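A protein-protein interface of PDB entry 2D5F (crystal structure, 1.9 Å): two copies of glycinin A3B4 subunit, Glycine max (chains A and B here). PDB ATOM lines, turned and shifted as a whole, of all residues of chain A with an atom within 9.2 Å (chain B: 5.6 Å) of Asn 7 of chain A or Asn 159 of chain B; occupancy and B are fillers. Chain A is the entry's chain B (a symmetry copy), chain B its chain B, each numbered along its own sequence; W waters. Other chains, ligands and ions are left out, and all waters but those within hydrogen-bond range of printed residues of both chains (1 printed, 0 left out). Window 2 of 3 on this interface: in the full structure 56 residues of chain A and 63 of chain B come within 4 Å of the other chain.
Water W1 lies within hydrogen-bond range of OD1 of CSD 406 of chain A (2.9 Å) and the guanidinium group (NE) of Arg 161 of chain B (3.2 Å).
The side-chain amide nitrogen of Asn 154 of chain B is in hydrogen-bond range of the backbone carbonyl oxygen of Asp 157 of chain B, at 3.0 Å. OD2 of Asp 157 of chain B sits close to OD1 of Asn 159 of chain B (3.1 Å). OD2 of Asp 157 of chain B is in salt-bridge range of NH2 of Arg 161 of chain B (2.7 Å). The backbone carbonyl oxygen of Asn 159 of chain B sits at hydrogen-bond distance from the guanidinium group of Arg 161 of chain B, 3.5 Å away. The side-chain amide oxygen of Gln 10 of chain A sits close to the side-chain amide oxygen of Asn 7 of chain A. SG of Cys 42 of chain A is disulfide-bonded to SG of Cys 9 of chain A, 2.0 Å away.
N of Cys 9 of chain A sits at hydrogen-bond distance from OD1 of Asp 157 of chain B (2.9 Å). The backbone NH of Gln 10 of chain A is in hydrogen-bond range of the side-chain carboxylate of Asp 157 of chain B. The side-chain amide oxygen (OD1) of Asn 159 of chain B lies close to the side-chain amide oxygen (OD1) of Asn 7 of chain A, at 2.5 Å. The side-chain amide nitrogen of Gln 10 of chain A sits close to the side-chain amide nitrogen of Asn 159 of chain B, 3.3 Å away. The guanidinium group of Arg 161 of chain B sits at hydrogen-bond distance from the backbone carbonyl oxygen of Cys 9 of chain A. OD1 of CSD 406 of chain A lies close to the guanidinium group (NE) of Arg 161 of chain B. NE2 of Gln 10 of chain A sits at hydrogen-bond distance from O of Thr 176 of chain B (2.9 Å).
No position is printed for both chains. Of the 10 pairs that touch across the chains among the printed residues, none has its exchanged pair printed and touching as well.
Of the 10 printed residues of chain A, 5 touch a printed residue of chain B. Among the printed residues, no Asp or Glu carboxylate lies within 4 Å of a Lys or Arg side-chain nitrogen of the other chain.
Asn 7 of chain A touches just these residues of chain B: Asp 157 (3.4 Å) and Asn 159 (2.5 Å). Of the printed residues of chain B, Glu 8 of chain A touches Asp 157. Printed residues of chain B within 4 Å of Gln 10 of chain A: Asp 157, Asn 159, Arg 161 and Thr 176. Of the printed residues of chain B, CSD 406 of chain A touches Arg 161. Asn 159 of chain B touches two residues of chain A. No residue of chain A comes within 4 Å of Pro 160 of chain B. Of the printed residues of chain A, Arg 161 of chain B touches Cys 9 (3.4 Å), Gln 10 (3.6 Å) and CSD 406 (3.7 Å). Of chain A, only Gln 10 comes within 4 Å of Thr 176 of chain B. The nearest printed residue of chain B that does not touch Gln 10 of chain A is Glu 175 of chain B (6.3 Å).
Asn 7 of chain A touches Asp 157 of chain B. Asp 157 of chain B touches Glu 8 of chain A. Gln 10 of chain A touches Arg 161 of chain B.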
ATOM      1  N   ASN A   7       2.246  -2.525  24.185  1.00  0.00           N
ATOM      2  CA  ASN A   7       2.949  -2.578  22.869  1.00  0.00           C
ATOM      3  C   ASN A   7       2.587  -3.862  22.132  1.00  0.00           C
ATOM      4  O   ASN A   7       3.385  -4.393  21.361  1.00  0.00           O
ATOM      5  CB  ASN A   7       4.467  -2.523  23.072  1.00  0.00           C
ATOM      6  CG  ASN A   7       4.902  -1.327  23.902  1.00  0.00           C
ATOM      7  OD1 ASN A   7       4.586  -0.182  23.577  1.00  0.00           O
ATOM      8  ND2 ASN A   7       5.635  -1.590  24.979  1.00  0.00           N
ATOM      9  N   GLU A   8       1.374  -4.345  22.369  1.00  0.00           N
ATOM     10  CA  GLU A   8       0.896  -5.573  21.750  1.00  0.00           C
ATOM     11  C   GLU A   8       0.919  -5.581  20.221  1.00  0.00           C
ATOM     12  O   GLU A   8       0.955  -6.645  19.610  1.00  0.00           O
ATOM     13  CB  GLU A   8      -0.517  -5.891  22.244  1.00  0.00           C
ATOM     14  CG  GLU A   8      -0.583  -6.224  23.736  1.00  0.00           C
ATOM     15  CD  GLU A   8      -0.728  -4.996  24.626  1.00  0.00           C
ATOM     16  OE1 GLU A   8       0.002  -3.998  24.423  1.00  0.00           O
ATOM     17  OE2 GLU A   8      -1.578  -5.038  25.543  1.00  0.00           O
ATOM     18  N   CYS A   9       0.898  -4.411  19.596  1.00  0.00           N
ATOM     19  CA  CYS A   9       0.924  -4.370  18.139  1.00  0.00           C
ATOM     20  C   CYS A   9       2.215  -3.825  17.541  1.00  0.00           C
ATOM     21  O   CYS A   9       2.269  -3.508  16.352  1.00  0.00           O
ATOM     22  CB  CYS A   9      -0.256  -3.571  17.593  1.00  0.00           C
ATOM     23  SG  CYS A   9      -1.889  -4.374  17.718  1.00  0.00           S
ATOM     24  N   GLN A  10       3.249  -3.694  18.360  1.00  0.00           N
ATOM     25  CA  GLN A  10       4.530  -3.229  17.843  1.00  0.00           C
ATOM     26  C   GLN A  10       5.225  -4.493  17.368  1.00  0.00           C
ATOM     27  O   GLN A  10       6.124  -5.006  18.022  1.00  0.00           O
ATOM     28  CB  GLN A  10       5.360  -2.555  18.933  1.00  0.00           C
ATOM     29  CG  GLN A  10       4.774  -1.255  19.440  1.00  0.00           C
ATOM     30  CD  GLN A  10       5.779  -0.435  20.227  1.00  0.00           C
ATOM     31  OE1 GLN A  10       6.252  -0.856  21.281  1.00  0.00           O
ATOM     32  NE2 GLN A  10       6.112   0.743  19.712  1.00  0.00           N
ATOM     33  N   LEU A  11       4.779  -5.006  16.232  1.00  0.00           N
ATOM     34  CA  LEU A  11       5.344  -6.227  15.684  1.00  0.00           C
ATOM     35  C   LEU A  11       6.233  -5.937  14.483  1.00  0.00           C
ATOM     36  O   LEU A  11       5.801  -5.318  13.513  1.00  0.00           O
ATOM     37  CB  LEU A  11       4.213  -7.177  15.287  1.00  0.00           C
ATOM     38  CG  LEU A  11       3.219  -7.506  16.406  1.00  0.00           C
ATOM     39  CD1 LEU A  11       2.137  -8.428  15.868  1.00  0.00           C
ATOM     40  CD2 LEU A  11       3.946  -8.159  17.572  1.00  0.00           C
ATOM     41  N   ASN A  12       7.479  -6.388  14.554  1.00  0.00           N
ATOM     42  CA  ASN A  12       8.426  -6.169  13.470  1.00  0.00           C
ATOM     43  C   ASN A  12       8.363  -7.305  12.469  1.00  0.00           C
ATOM     44  O   ASN A  12       8.977  -7.248  11.404  1.00  0.00           O
ATOM     45  CB  ASN A  12       9.836  -6.036  14.032  1.00  0.00           C
ATOM     46  CG  ASN A  12       9.955  -4.890  15.013  1.00  0.00           C
ATOM     47  OD1 ASN A  12       9.674  -3.734  14.675  1.00  0.00           O
ATOM     48  ND2 ASN A  12      10.364  -5.200  16.241  1.00  0.00           N
ATOM     49  N   PRO A  38       1.699 -13.638  19.062  1.00  0.00           N
ATOM     50  CA  PRO A  38       1.679 -12.175  19.146  1.00  0.00           C
ATOM     51  C   PRO A  38       0.793 -11.466  18.118  1.00  0.00           C
ATOM     52  O   PRO A  38       0.202 -10.429  18.422  1.00  0.00           O
ATOM     53  CB  PRO A  38       3.168 -11.786  19.040  1.00  0.00           C
ATOM     54  CG  PRO A  38       3.855 -13.033  18.522  1.00  0.00           C
ATOM     55  CD  PRO A  38       3.076 -14.153  19.142  1.00  0.00           C
ATOM     56  N   GLN A  41      -2.723 -11.669  19.385  1.00  0.00           N
ATOM     57  CA  GLN A  41      -2.906 -10.873  20.589  1.00  0.00           C
ATOM     58  C   GLN A  41      -3.075  -9.415  20.185  1.00  0.00           C
ATOM     59  O   GLN A  41      -3.842  -8.680  20.799  1.00  0.00           O
ATOM     60  CB  GLN A  41      -1.711 -11.011  21.532  1.00  0.00           C
ATOM     61  CG  GLN A  41      -1.549 -12.405  22.091  1.00  0.00           C
ATOM     62  CD  GLN A  41      -0.595 -12.444  23.251  1.00  0.00           C
ATOM     63  OE1 GLN A  41       0.576 -12.086  23.117  1.00  0.00           O
ATOM     64  NE2 GLN A  41      -1.086 -12.875  24.406  1.00  0.00           N
ATOM     65  N   CYS A  42      -2.361  -9.004  19.143  1.00  0.00           N
ATOM     66  CA  CYS A  42      -2.462  -7.635  18.660  1.00  0.00           C
ATOM     67  C   CYS A  42      -3.868  -7.405  18.089  1.00  0.00           C
ATOM     68  O   CYS A  42      -4.482  -6.362  18.316  1.00  0.00           O
ATOM     69  CB  CYS A  42      -1.383  -7.366  17.594  1.00  0.00           C
ATOM     70  SG  CYS A  42      -1.774  -5.981  16.477  1.00  0.00           S
ATOM     71  N   CSD A 406       4.270   1.508  10.018  1.00  0.00           N
ATOM     72  CA  CSD A 406       4.493   2.954  10.031  1.00  0.00           C
ATOM     73  CB  CSD A 406       3.872   3.582  11.288  1.00  0.00           C
ATOM     74  SG  CSD A 406       4.346   2.848  12.873  1.00  0.00           S
ATOM     75  C   CSD A 406       5.947   3.407   9.882  1.00  0.00           C
ATOM     76  O   CSD A 406       6.225   4.606   9.823  1.00  0.00           O
ATOM     77  OD1 CSD A 406       3.901   1.433  12.863  1.00  0.00           O
ATOM     78  OD2 CSD A 406       5.804   2.978  12.981  1.00  0.00           O
ATOM     79  N   SER B  35       5.211  10.420  25.397  1.00  0.00           N
ATOM     80  CA  SER B  35       3.939   9.840  25.825  1.00  0.00           C
ATOM     81  C   SER B  35       4.048   9.013  27.111  1.00  0.00           C
ATOM     82  O   SER B  35       3.039   8.582  27.662  1.00  0.00           O
ATOM     83  CB  SER B  35       3.349   8.973  24.705  1.00  0.00           C
ATOM     84  OG  SER B  35       4.203   7.883  24.413  1.00  0.00           O
ATOM     85  N   TYR B  65      -5.858   7.114  15.272  1.00  0.00           N
ATOM     86  CA  TYR B  65      -6.648   7.707  16.350  1.00  0.00           C
ATOM     87  C   TYR B  65      -6.939   9.138  15.940  1.00  0.00           C
ATOM     88  O   TYR B  65      -6.285   9.677  15.058  1.00  0.00           O
ATOM     89  CB  TYR B  65      -5.888   7.683  17.687  1.00  0.00           C
ATOM     90  CG  TYR B  65      -4.414   8.011  17.560  1.00  0.00           C
ATOM     91  CD1 TYR B  65      -3.457   6.993  17.480  1.00  0.00           C
ATOM     92  CD2 TYR B  65      -3.978   9.334  17.472  1.00  0.00           C
ATOM     93  CE1 TYR B  65      -2.103   7.284  17.314  1.00  0.00           C
ATOM     94  CE2 TYR B  65      -2.629   9.637  17.303  1.00  0.00           C
ATOM     95  CZ  TYR B  65      -1.696   8.606  17.222  1.00  0.00           C
ATOM     96  OH  TYR B  65      -0.362   8.903  17.032  1.00  0.00           O
ATOM     97  N   THR B 149      -4.441   8.969  21.599  1.00  0.00           N
ATOM     98  CA  THR B 149      -3.993   7.582  21.469  1.00  0.00           C
ATOM     99  C   THR B 149      -4.874   6.542  22.167  1.00  0.00           C
ATOM    100  O   THR B 149      -4.985   5.414  21.698  1.00  0.00           O
ATOM    101  CB  THR B 149      -2.557   7.398  22.016  1.00  0.00           C
ATOM    102  OG1 THR B 149      -2.469   7.979  23.323  1.00  0.00           O
ATOM    103  CG2 THR B 149      -1.532   8.056  21.099  1.00  0.00           C
ATOM    104  N   ASN B 154      -8.766   3.281  18.306  1.00  0.00           N
ATOM    105  CA  ASN B 154      -7.393   2.822  18.100  1.00  0.00           C
ATOM    106  C   ASN B 154      -7.314   1.380  18.580  1.00  0.00           C
ATOM    107  O   ASN B 154      -7.297   1.115  19.778  1.00  0.00           O
ATOM    108  CB  ASN B 154      -6.407   3.705  18.880  1.00  0.00           C
ATOM    109  CG  ASN B 154      -4.963   3.235  18.749  1.00  0.00           C
ATOM    110  OD1 ASN B 154      -4.650   2.342  17.956  1.00  0.00           O
ATOM    111  ND2 ASN B 154      -4.080   3.838  19.526  1.00  0.00           N
ATOM    112  N   ASP B 157      -2.256  -0.215  19.892  1.00  0.00           N
ATOM    113  CA  ASP B 157      -1.840  -0.139  21.288  1.00  0.00           C
ATOM    114  C   ASP B 157      -1.675   1.332  21.629  1.00  0.00           C
ATOM    115  O   ASP B 157      -1.889   2.184  20.775  1.00  0.00           O
ATOM    116  CB  ASP B 157      -0.558  -0.936  21.568  1.00  0.00           C
ATOM    117  CG  ASP B 157       0.562  -0.609  20.619  1.00  0.00           C
ATOM    118  OD1 ASP B 157       1.171  -1.567  20.098  1.00  0.00           O
ATOM    119  OD2 ASP B 157       0.839   0.585  20.399  1.00  0.00           O
ATOM    120  N   GLN B 158      -1.293   1.626  22.865  1.00  0.00           N
ATOM    121  CA  GLN B 158      -1.172   3.008  23.327  1.00  0.00           C
ATOM    122  C   GLN B 158      -0.131   3.892  22.651  1.00  0.00           C
ATOM    123  O   GLN B 158      -0.156   5.108  22.819  1.00  0.00           O
ATOM    124  CB  GLN B 158      -0.925   3.020  24.837  1.00  0.00           C
ATOM    125  CG  GLN B 158       0.522   2.783  25.227  1.00  0.00           C
ATOM    126  CD  GLN B 158       1.153   4.021  25.825  1.00  0.00           C
ATOM    127  OE1 GLN B 158       0.761   4.471  26.905  1.00  0.00           O
ATOM    128  NE2 GLN B 158       2.133   4.588  25.123  1.00  0.00           N
ATOM    129  N   ASN B 159       0.781   3.301  21.889  1.00  0.00           N
ATOM    130  CA  ASN B 159       1.817   4.098  21.244  1.00  0.00           C
ATOM    131  C   ASN B 159       1.319   5.012  20.136  1.00  0.00           C
ATOM    132  O   ASN B 159       0.428   4.654  19.366  1.00  0.00           O
ATOM    133  CB  ASN B 159       2.906   3.207  20.641  1.00  0.00           C
ATOM    134  CG  ASN B 159       3.662   2.409  21.684  1.00  0.00           C
ATOM    135  OD1 ASN B 159       3.153   1.426  22.220  1.00  0.00           O
ATOM    136  ND2 ASN B 159       4.885   2.831  21.975  1.00  0.00           N
ATOM    137  N   PRO B 160       1.884   6.224  20.056  1.00  0.00           N
ATOM    138  CA  PRO B 160       1.477   7.150  19.001  1.00  0.00           C
ATOM    139  C   PRO B 160       2.136   6.606  17.733  1.00  0.00           C
ATOM    140  O   PRO B 160       3.219   6.015  17.796  1.00  0.00           O
ATOM    141  CB  PRO B 160       2.067   8.482  19.463  1.00  0.00           C
ATOM    142  CG  PRO B 160       3.257   8.073  20.278  1.00  0.00           C
ATOM    143  CD  PRO B 160       2.733   6.898  21.055  1.00  0.00           C
ATOM    144  N   ARG B 161       1.479   6.768  16.592  1.00  0.00           N
ATOM    145  CA  ARG B 161       2.023   6.267  15.333  1.00  0.00           C
ATOM    146  C   ARG B 161       1.657   7.216  14.209  1.00  0.00           C
ATOM    147  O   ARG B 161       0.534   7.712  14.164  1.00  0.00           O
ATOM    148  CB  ARG B 161       1.430   4.898  14.974  1.00  0.00           C
ATOM    149  CG  ARG B 161       1.796   3.718  15.854  1.00  0.00           C
ATOM    150  CD  ARG B 161       1.154   2.467  15.268  1.00  0.00           C
ATOM    151  NE  ARG B 161       1.663   1.222  15.841  1.00  0.00           N
ATOM    152  CZ  ARG B 161       1.404   0.798  17.073  1.00  0.00           C
ATOM    153  NH1 ARG B 161       1.916  -0.351  17.498  1.00  0.00           N
ATOM    154  NH2 ARG B 161       0.632   1.519  17.880  1.00  0.00           N
ATOM    155  N   GLU B 175      10.329   7.653  21.882  1.00  0.00           N
ATOM    156  CA  GLU B 175      10.108   6.809  23.043  1.00  0.00           C
ATOM    157  C   GLU B 175       9.432   5.489  22.669  1.00  0.00           C
ATOM    158  O   GLU B 175       9.479   4.534  23.439  1.00  0.00           O
ATOM    159  CB  GLU B 175       9.269   7.541  24.097  1.00  0.00           C
ATOM    160  CG  GLU B 175       7.773   7.637  23.800  1.00  0.00           C
ATOM    161  CD  GLU B 175       7.394   8.845  22.964  1.00  0.00           C
ATOM    162  OE1 GLU B 175       6.182   9.144  22.901  1.00  0.00           O
ATOM    163  OE2 GLU B 175       8.288   9.491  22.371  1.00  0.00           O
ATOM    164  N   THR B 176       8.822   5.429  21.485  1.00  0.00           N
ATOM    165  CA  THR B 176       8.141   4.209  21.046  1.00  0.00           C
ATOM    166  C   THR B 176       9.067   3.190  20.385  1.00  0.00           C
ATOM    167  O   THR B 176       8.692   2.029  20.209  1.00  0.00           O
ATOM    168  CB  THR B 176       6.998   4.505  20.039  1.00  0.00           C
ATOM    169  OG1 THR B 176       7.546   5.073  18.842  1.00  0.00           O
ATOM    170  CG2 THR B 176       5.975   5.459  20.644  1.00  0.00           C
HETATM  171  O   HOH W   1       4.077  -0.620  14.891  1.00  0.00           O
